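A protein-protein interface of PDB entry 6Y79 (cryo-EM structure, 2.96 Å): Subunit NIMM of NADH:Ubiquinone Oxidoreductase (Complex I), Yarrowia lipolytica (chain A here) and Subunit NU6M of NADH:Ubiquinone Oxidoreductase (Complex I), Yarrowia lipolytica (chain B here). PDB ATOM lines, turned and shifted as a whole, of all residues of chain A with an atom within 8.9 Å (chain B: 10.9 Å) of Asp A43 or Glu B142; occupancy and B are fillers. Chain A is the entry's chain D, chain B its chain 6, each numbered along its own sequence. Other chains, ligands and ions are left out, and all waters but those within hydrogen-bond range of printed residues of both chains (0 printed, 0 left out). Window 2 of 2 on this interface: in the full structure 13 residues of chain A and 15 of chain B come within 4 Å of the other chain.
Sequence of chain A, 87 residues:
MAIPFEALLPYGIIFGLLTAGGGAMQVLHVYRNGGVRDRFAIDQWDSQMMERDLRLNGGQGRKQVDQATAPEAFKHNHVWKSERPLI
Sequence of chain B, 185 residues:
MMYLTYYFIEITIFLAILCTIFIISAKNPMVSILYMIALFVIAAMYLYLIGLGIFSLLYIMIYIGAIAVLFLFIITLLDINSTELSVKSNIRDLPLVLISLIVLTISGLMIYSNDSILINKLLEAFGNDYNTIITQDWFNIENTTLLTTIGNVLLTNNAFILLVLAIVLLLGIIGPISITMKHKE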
ATOM      1  N   ARG A  39     -21.177 -35.872  41.014  1.00  0.00           N
ATOM      2  CA  ARG A  39     -21.469 -35.761  39.595  1.00  0.00           C
ATOM      3  C   ARG A  39     -20.332 -34.983  38.953  1.00  0.00           C
ATOM      4  O   ARG A  39     -20.119 -33.810  39.272  1.00  0.00           O
ATOM      5  CB  ARG A  39     -22.799 -35.060  39.380  1.00  0.00           C
ATOM      6  CG  ARG A  39     -23.957 -35.679  40.106  1.00  0.00           C
ATOM      7  CD  ARG A  39     -25.180 -34.895  39.745  1.00  0.00           C
ATOM      8  NE  ARG A  39     -25.158 -34.657  38.310  1.00  0.00           N
ATOM      9  CZ  ARG A  39     -25.968 -35.243  37.447  1.00  0.00           C
ATOM     10  NH1 ARG A  39     -26.897 -36.061  37.884  1.00  0.00           N
ATOM     11  NH2 ARG A  39     -25.863 -34.992  36.154  1.00  0.00           N
ATOM     12  N   PHE A  40     -19.605 -35.629  38.047  1.00  0.00           N
ATOM     13  CA  PHE A  40     -18.322 -35.091  37.633  1.00  0.00           C
ATOM     14  C   PHE A  40     -18.382 -34.265  36.355  1.00  0.00           C
ATOM     15  O   PHE A  40     -17.380 -33.638  36.004  1.00  0.00           O
ATOM     16  CB  PHE A  40     -17.291 -36.228  37.503  1.00  0.00           C
ATOM     17  CG  PHE A  40     -17.616 -37.264  36.459  1.00  0.00           C
ATOM     18  CD1 PHE A  40     -17.199 -37.107  35.146  1.00  0.00           C
ATOM     19  CD2 PHE A  40     -18.283 -38.424  36.806  1.00  0.00           C
ATOM     20  CE1 PHE A  40     -17.486 -38.051  34.194  1.00  0.00           C
ATOM     21  CE2 PHE A  40     -18.563 -39.379  35.856  1.00  0.00           C
ATOM     22  CZ  PHE A  40     -18.165 -39.190  34.549  1.00  0.00           C
ATOM     23  N   ALA A  41     -19.509 -34.238  35.652  1.00  0.00           N
ATOM     24  CA  ALA A  41     -19.632 -33.401  34.459  1.00  0.00           C
ATOM     25  C   ALA A  41     -21.096 -33.035  34.315  1.00  0.00           C
ATOM     26  O   ALA A  41     -21.904 -33.882  33.929  1.00  0.00           O
ATOM     27  CB  ALA A  41     -19.131 -34.122  33.213  1.00  0.00           C
ATOM     28  N   ILE A  42     -21.447 -31.794  34.613  1.00  0.00           N
ATOM     29  CA  ILE A  42     -22.848 -31.417  34.700  1.00  0.00           C
ATOM     30  C   ILE A  42     -23.180 -30.446  33.581  1.00  0.00           C
ATOM     31  O   ILE A  42     -22.684 -29.313  33.535  1.00  0.00           O
ATOM     32  CB  ILE A  42     -23.205 -30.843  36.070  1.00  0.00           C
ATOM     33  CG1 ILE A  42     -23.053 -31.927  37.127  1.00  0.00           C
ATOM     34  CG2 ILE A  42     -24.635 -30.382  36.084  1.00  0.00           C
ATOM     35  CD1 ILE A  42     -23.130 -31.403  38.518  1.00  0.00           C
ATOM     36  N   ASP A  43     -24.058 -30.913  32.705  1.00  0.00           N
ATOM     37  CA  ASP A  43     -24.713 -30.181  31.639  1.00  0.00           C
ATOM     38  C   ASP A  43     -25.501 -28.977  32.153  1.00  0.00           C
ATOM     39  O   ASP A  43     -25.716 -28.804  33.348  1.00  0.00           O
ATOM     40  CB  ASP A  43     -25.657 -31.143  30.933  1.00  0.00           C
ATOM     41  CG  ASP A  43     -25.899 -30.782  29.503  1.00  0.00           C
ATOM     42  OD1 ASP A  43     -25.363 -29.752  29.062  1.00  0.00           O
ATOM     43  OD2 ASP A  43     -26.587 -31.562  28.827  1.00  0.00           O
ATOM     44  N   GLN A  44     -25.936 -28.132  31.219  1.00  0.00           N
ATOM     45  CA  GLN A  44     -26.969 -27.153  31.539  1.00  0.00           C
ATOM     46  C   GLN A  44     -28.288 -27.854  31.835  1.00  0.00           C
ATOM     47  O   GLN A  44     -29.019 -27.475  32.760  1.00  0.00           O
ATOM     48  CB  GLN A  44     -27.120 -26.161  30.385  1.00  0.00           C
ATOM     49  CG  GLN A  44     -28.354 -25.263  30.442  1.00  0.00           C
ATOM     50  CD  GLN A  44     -28.407 -24.293  29.281  1.00  0.00           C
ATOM     51  OE1 GLN A  44     -27.655 -24.424  28.320  1.00  0.00           O
ATOM     52  NE2 GLN A  44     -29.306 -23.321  29.354  1.00  0.00           N
ATOM     53  N   TRP A  45     -28.582 -28.903  31.062  1.00  0.00           N
ATOM     54  CA  TRP A  45     -29.767 -29.731  31.278  1.00  0.00           C
ATOM     55  C   TRP A  45     -29.741 -30.399  32.642  1.00  0.00           C
ATOM     56  O   TRP A  45     -30.745 -30.400  33.359  1.00  0.00           O
ATOM     57  CB  TRP A  45     -29.849 -30.786  30.179  1.00  0.00           C
ATOM     58  CG  TRP A  45     -30.990 -31.741  30.279  1.00  0.00           C
ATOM     59  CD1 TRP A  45     -31.009 -32.940  30.923  1.00  0.00           C
ATOM     60  CD2 TRP A  45     -32.270 -31.597  29.668  1.00  0.00           C
ATOM     61  NE1 TRP A  45     -32.231 -33.541  30.771  1.00  0.00           N
ATOM     62  CE2 TRP A  45     -33.024 -32.735  30.001  1.00  0.00           C
ATOM     63  CE3 TRP A  45     -32.859 -30.605  28.886  1.00  0.00           C
ATOM     64  CZ2 TRP A  45     -34.332 -32.908  29.575  1.00  0.00           C
ATOM     65  CZ3 TRP A  45     -34.146 -30.781  28.459  1.00  0.00           C
ATOM     66  CH2 TRP A  45     -34.875 -31.921  28.806  1.00  0.00           C
ATOM     67  N   ASP A  46     -28.599 -30.963  33.028  1.00  0.00           N
ATOM     68  CA  ASP A  46     -28.527 -31.633  34.319  1.00  0.00           C
ATOM     69  C   ASP A  46     -28.447 -30.638  35.470  1.00  0.00           C
ATOM     70  O   ASP A  46     -28.872 -30.952  36.582  1.00  0.00           O
ATOM     71  CB  ASP A  46     -27.350 -32.592  34.348  1.00  0.00           C
ATOM     72  CG  ASP A  46     -27.645 -33.887  33.623  1.00  0.00           C
ATOM     73  OD1 ASP A  46     -28.574 -34.613  34.040  1.00  0.00           O
ATOM     74  OD2 ASP A  46     -26.945 -34.180  32.633  1.00  0.00           O
ATOM     75  N   SER A  47     -27.926 -29.432  35.222  1.00  0.00           N
ATOM     76  CA  SER A  47     -28.033 -28.356  36.205  1.00  0.00           C
ATOM     77  C   SER A  47     -29.494 -28.005  36.481  1.00  0.00           C
ATOM     78  O   SER A  47     -29.913 -27.897  37.648  1.00  0.00           O
ATOM     79  CB  SER A  47     -27.283 -27.118  35.715  1.00  0.00           C
ATOM     80  OG  SER A  47     -25.905 -27.371  35.509  1.00  0.00           O
ATOM     81  N   GLN A  48     -30.286 -27.854  35.412  1.00  0.00           N
ATOM     82  CA  GLN A  48     -31.714 -27.585  35.562  1.00  0.00           C
ATOM     83  C   GLN A  48     -32.440 -28.772  36.180  1.00  0.00           C
ATOM     84  O   GLN A  48     -33.435 -28.617  36.896  1.00  0.00           O
ATOM     85  CB  GLN A  48     -32.320 -27.233  34.213  1.00  0.00           C
ATOM     86  CG  GLN A  48     -31.901 -25.901  33.677  1.00  0.00           C
ATOM     87  CD  GLN A  48     -32.526 -25.618  32.340  1.00  0.00           C
ATOM     88  OE1 GLN A  48     -33.253 -26.441  31.799  1.00  0.00           O
ATOM     89  NE2 GLN A  48     -32.247 -24.447  31.798  1.00  0.00           N
ATOM     90  N   MET A  49     -31.943 -29.967  35.937  1.00  0.00           N
ATOM     91  CA  MET A  49     -32.585 -31.147  36.505  1.00  0.00           C
ATOM     92  C   MET A  49     -32.299 -31.276  37.999  1.00  0.00           C
ATOM     93  O   MET A  49     -33.183 -31.654  38.784  1.00  0.00           O
ATOM     94  CB  MET A  49     -32.134 -32.393  35.754  1.00  0.00           C
ATOM     95  CG  MET A  49     -33.008 -33.531  36.035  1.00  0.00           C
ATOM     96  SD  MET A  49     -34.727 -33.273  35.594  1.00  0.00           S
ATOM     97  CE  MET A  49     -34.591 -33.557  33.851  1.00  0.00           C
ATOM     98  N   MET A  50     -31.085 -30.906  38.418  1.00  0.00           N
ATOM     99  CA  MET A  50     -30.735 -30.904  39.834  1.00  0.00           C
ATOM    100  C   MET A  50     -31.525 -29.863  40.618  1.00  0.00           C
ATOM    101  O   MET A  50     -31.952 -30.132  41.744  1.00  0.00           O
ATOM    102  CB  MET A  50     -29.239 -30.669  40.008  1.00  0.00           C
ATOM    103  CG  MET A  50     -28.393 -31.869  39.695  1.00  0.00           C
ATOM    104  SD  MET A  50     -26.644 -31.469  39.744  1.00  0.00           S
ATOM    105  CE  MET A  50     -26.361 -31.487  41.507  1.00  0.00           C
ATOM    106  N   ASP B 137     -36.331 -22.978  29.942  1.00  0.00           N
ATOM    107  CA  ASP B 137     -36.991 -23.780  28.933  1.00  0.00           C
ATOM    108  C   ASP B 137     -36.142 -25.014  28.679  1.00  0.00           C
ATOM    109  O   ASP B 137     -34.911 -24.937  28.674  1.00  0.00           O
ATOM    110  CB  ASP B 137     -37.207 -22.970  27.661  1.00  0.00           C
ATOM    111  CG  ASP B 137     -35.927 -22.413  27.117  1.00  0.00           C
ATOM    112  OD1 ASP B 137     -35.310 -21.570  27.801  1.00  0.00           O
ATOM    113  OD2 ASP B 137     -35.531 -22.812  26.007  1.00  0.00           O
ATOM    114  N   TRP B 138     -36.804 -26.151  28.494  1.00  0.00           N
ATOM    115  CA  TRP B 138     -36.158 -27.458  28.408  1.00  0.00           C
ATOM    116  C   TRP B 138     -35.970 -27.908  26.970  1.00  0.00           C
ATOM    117  O   TRP B 138     -36.156 -29.082  26.669  1.00  0.00           O
ATOM    118  CB  TRP B 138     -36.968 -28.501  29.177  1.00  0.00           C
ATOM    119  CG  TRP B 138     -37.066 -28.285  30.655  1.00  0.00           C
ATOM    120  CD1 TRP B 138     -38.004 -27.558  31.307  1.00  0.00           C
ATOM    121  CD2 TRP B 138     -36.215 -28.839  31.666  1.00  0.00           C
ATOM    122  NE1 TRP B 138     -37.783 -27.602  32.658  1.00  0.00           N
ATOM    123  CE2 TRP B 138     -36.689 -28.383  32.904  1.00  0.00           C
ATOM    124  CE3 TRP B 138     -35.089 -29.665  31.641  1.00  0.00           C
ATOM    125  CZ2 TRP B 138     -36.085 -28.723  34.102  1.00  0.00           C
ATOM    126  CZ3 TRP B 138     -34.492 -30.000  32.828  1.00  0.00           C
ATOM    127  CH2 TRP B 138     -34.995 -29.539  34.044  1.00  0.00           C
ATOM    128  N   PHE B 139     -35.638 -27.008  26.049  1.00  0.00           N
ATOM    129  CA  PHE B 139     -35.596 -27.359  24.634  1.00  0.00           C
ATOM    130  C   PHE B 139     -34.240 -27.861  24.155  1.00  0.00           C
ATOM    131  O   PHE B 139     -34.153 -28.350  23.026  1.00  0.00           O
ATOM    132  CB  PHE B 139     -35.990 -26.161  23.769  1.00  0.00           C
ATOM    133  CG  PHE B 139     -37.423 -25.753  23.898  1.00  0.00           C
ATOM    134  CD1 PHE B 139     -38.431 -26.517  23.340  1.00  0.00           C
ATOM    135  CD2 PHE B 139     -37.756 -24.579  24.545  1.00  0.00           C
ATOM    136  CE1 PHE B 139     -39.748 -26.124  23.448  1.00  0.00           C
ATOM    137  CE2 PHE B 139     -39.067 -24.181  24.656  1.00  0.00           C
ATOM    138  CZ  PHE B 139     -40.063 -24.952  24.103  1.00  0.00           C
ATOM    139  N   ASN B 140     -33.187 -27.753  24.959  1.00  0.00           N
ATOM    140  CA  ASN B 140     -31.831 -28.080  24.532  1.00  0.00           C
ATOM    141  C   ASN B 140     -31.336 -29.327  25.250  1.00  0.00           C
ATOM    142  O   ASN B 140     -31.299 -29.361  26.480  1.00  0.00           O
ATOM    143  CB  ASN B 140     -30.884 -26.915  24.807  1.00  0.00           C
ATOM    144  CG  ASN B 140     -29.511 -27.129  24.216  1.00  0.00           C
ATOM    145  OD1 ASN B 140     -29.327 -27.945  23.314  1.00  0.00           O
ATOM    146  ND2 ASN B 140     -28.531 -26.405  24.734  1.00  0.00           N
ATOM    147  N   ILE B 141     -30.903 -30.324  24.484  1.00  0.00           N
ATOM    148  CA  ILE B 141     -30.662 -31.664  25.003  1.00  0.00           C
ATOM    149  C   ILE B 141     -29.192 -31.994  25.177  1.00  0.00           C
ATOM    150  O   ILE B 141     -28.881 -33.106  25.623  1.00  0.00           O
ATOM    151  CB  ILE B 141     -31.333 -32.724  24.112  1.00  0.00           C
ATOM    152  CG1 ILE B 141     -31.001 -32.442  22.652  1.00  0.00           C
ATOM    153  CG2 ILE B 141     -32.800 -32.708  24.317  1.00  0.00           C
ATOM    154  CD1 ILE B 141     -31.647 -33.369  21.678  1.00  0.00           C
ATOM    155  N   GLU B 142     -28.272 -31.089  24.855  1.00  0.00           N
ATOM    156  CA  GLU B 142     -26.873 -31.491  24.891  1.00  0.00           C
ATOM    157  C   GLU B 142     -25.964 -30.343  25.295  1.00  0.00           C
ATOM    158  O   GLU B 142     -26.362 -29.177  25.309  1.00  0.00           O
ATOM    159  CB  GLU B 142     -26.426 -32.045  23.550  1.00  0.00           C
ATOM    160  CG  GLU B 142     -26.756 -31.166  22.392  1.00  0.00           C
ATOM    161  CD  GLU B 142     -26.229 -31.746  21.111  1.00  0.00           C
ATOM    162  OE1 GLU B 142     -25.856 -32.937  21.116  1.00  0.00           O
ATOM    163  OE2 GLU B 142     -26.171 -31.014  20.104  1.00  0.00           O
ATOM    164  N   ASN B 143     -24.716 -30.699  25.606  1.00  0.00           N
ATOM    165  CA  ASN B 143     -23.748 -29.765  26.175  1.00  0.00           C
ATOM    166  C   ASN B 143     -23.035 -29.006  25.059  1.00  0.00           C
ATOM    167  O   ASN B 143     -21.813 -29.037  24.906  1.00  0.00           O
ATOM    168  CB  ASN B 143     -22.762 -30.505  27.067  1.00  0.00           C
ATOM    169  CG  ASN B 143     -22.208 -29.630  28.176  1.00  0.00           C
ATOM    170  OD1 ASN B 143     -22.695 -28.527  28.419  1.00  0.00           O
ATOM    171  ND2 ASN B 143     -21.185 -30.128  28.861  1.00  0.00           N
ATOM    172  N   THR B 144     -23.833 -28.312  24.264  1.00  0.00           N
ATOM    173  CA  THR B 144     -23.277 -27.320  23.364  1.00  0.00           C
ATOM    174  C   THR B 144     -23.036 -26.066  24.181  1.00  0.00           C
ATOM    175  O   THR B 144     -23.948 -25.275  24.419  1.00  0.00           O
ATOM    176  CB  THR B 144     -24.210 -27.055  22.194  1.00  0.00           C
ATOM    177  OG1 THR B 144     -24.525 -28.290  21.547  1.00  0.00           O
ATOM    178  CG2 THR B 144     -23.511 -26.166  21.205  1.00  0.00           C
ATOM    179  N   THR B 145     -21.810 -25.899  24.648  1.00  0.00           N
ATOM    180  CA  THR B 145     -21.443 -24.641  25.259  1.00  0.00           C
ATOM    181  C   THR B 145     -20.951 -23.688  24.178  1.00  0.00           C
ATOM    182  O   THR B 145     -21.068 -23.948  22.980  1.00  0.00           O
ATOM    183  CB  THR B 145     -20.397 -24.850  26.351  1.00  0.00           C
ATOM    184  OG1 THR B 145     -19.182 -25.340  25.774  1.00  0.00           O
ATOM    185  CG2 THR B 145     -20.907 -25.835  27.377  1.00  0.00           C
ATOM    186  N   LEU B 146     -20.382 -22.574  24.615  1.00  0.00           N
ATOM    187  CA  LEU B 146     -20.127 -21.459  23.716  1.00  0.00           C
ATOM    188  C   LEU B 146     -18.950 -21.737  22.786  1.00  0.00           C
ATOM    189  O   LEU B 146     -18.955 -21.312  21.624  1.00  0.00           O
ATOM    190  CB  LEU B 146     -19.901 -20.209  24.557  1.00  0.00           C
ATOM    191  CG  LEU B 146     -19.629 -18.866  23.919  1.00  0.00           C
ATOM    192  CD1 LEU B 146     -20.386 -17.831  24.679  1.00  0.00           C
ATOM    193  CD2 LEU B 146     -18.170 -18.610  24.045  1.00  0.00           C
ATOM    194  N   THR B 148     -18.147 -24.634  21.614  1.00  0.00           N
ATOM    195  CA  THR B 148     -18.648 -25.542  20.592  1.00  0.00           C
ATOM    196  C   THR B 148     -19.330 -24.791  19.457  1.00  0.00           C
ATOM    197  O   THR B 148     -19.122 -25.108  18.281  1.00  0.00           O
ATOM    198  CB  THR B 148     -19.611 -26.542  21.223  1.00  0.00           C
ATOM    199  OG1 THR B 148     -18.929 -27.275  22.246  1.00  0.00           O
ATOM    200  CG2 THR B 148     -20.129 -27.512  20.183  1.00  0.00           C
ATOM    201  N   THR B 149     -20.128 -23.771  19.777  1.00  0.00           N
ATOM    202  CA  THR B 149     -20.818 -23.058  18.713  1.00  0.00           C
ATOM    203  C   THR B 149     -19.868 -22.131  17.967  1.00  0.00           C
ATOM    204  O   THR B 149     -20.039 -21.922  16.759  1.00  0.00           O
ATOM    205  CB  THR B 149     -22.007 -22.291  19.278  1.00  0.00           C
ATOM    206  OG1 THR B 149     -22.705 -23.139  20.190  1.00  0.00           O
ATOM    207  CG2 THR B 149     -22.953 -21.893  18.144  1.00  0.00           C
ATOM    208  N   ASN B 152     -18.497 -24.358  15.570  1.00  0.00           N
ATOM    209  CA  ASN B 152     -19.385 -24.728  14.474  1.00  0.00           C
ATOM    210  C   ASN B 152     -19.462 -23.630  13.438  1.00  0.00           C
ATOM    211  O   ASN B 152     -19.488 -23.915  12.241  1.00  0.00           O
ATOM    212  CB  ASN B 152     -20.796 -25.035  14.992  1.00  0.00           C
ATOM    213  CG  ASN B 152     -21.690 -25.738  13.966  1.00  0.00           C
ATOM    214  OD1 ASN B 152     -21.268 -26.071  12.858  1.00  0.00           O
ATOM    215  ND2 ASN B 152     -22.959 -25.924  14.324  1.00  0.00           N
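Of the 12 printed residues of chain A, 4 touch a printed residue of chain B.
Hydrophobic or aromatic side chains of chain A within 4 Å of the printed part of chain B: Trp A45 and Met A49.
Along chain B the printed residues that touch a printed residue of chain A span positions 137 to 143.
Among the printed residues, merely in contact across the chains: Asp A43 with Glu B142 (3.8 Å), Trp A45 with Trp B138 (3.2 Å), Trp A45 with Asn B140 (3.1 Å), Gln A48 with Asp B137 (3.8 Å), Gln A48 with Trp B138 (3.4 Å) and Met A49 with Trp B138 (3.6 Å).
Glu B142 touches just one residue of chain A: Asp A43 (3.8 Å).
No residue of chain B comes within 4 Å of Ala A41.
No residue of chain B comes within 4 Å of Ile A42.
No residue of chain B comes within 4 Å of Ser A47.
Of chain A, only Asp A43 (3.0 Å) comes within 4 Å of Asn B143.
Of the printed residues of chain A, Trp B138 touches Trp A45 (3.2 Å), Gln A48 (3.4 Å) and Met A49 (3.6 Å).
Printed residues of chain B within 4 Å of Gln A48: Asp B137 and Trp B138.
Of the printed residues of chain B, Trp A45 touches Trp B138 and Asn B140.
Of the printed residues of chain A, Asn B140 touches Trp A45 (3.1 Å).
Phe B139 touches none of the printed residues of chain A.
The side-chain carboxylate (OD1) of Asp A43 sits close to the side-chain amide oxygen (OD1) of Asn B143, at 3.0 Å.
The side-chain carboxylate (OE2) of Glu B142 lies within hydrogen-bond range of the side-chain hydroxyl (OG1) of Thr B144.
O of Asp A43 lies within hydrogen-bond range of OG of Ser A47 (2.6 Å).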
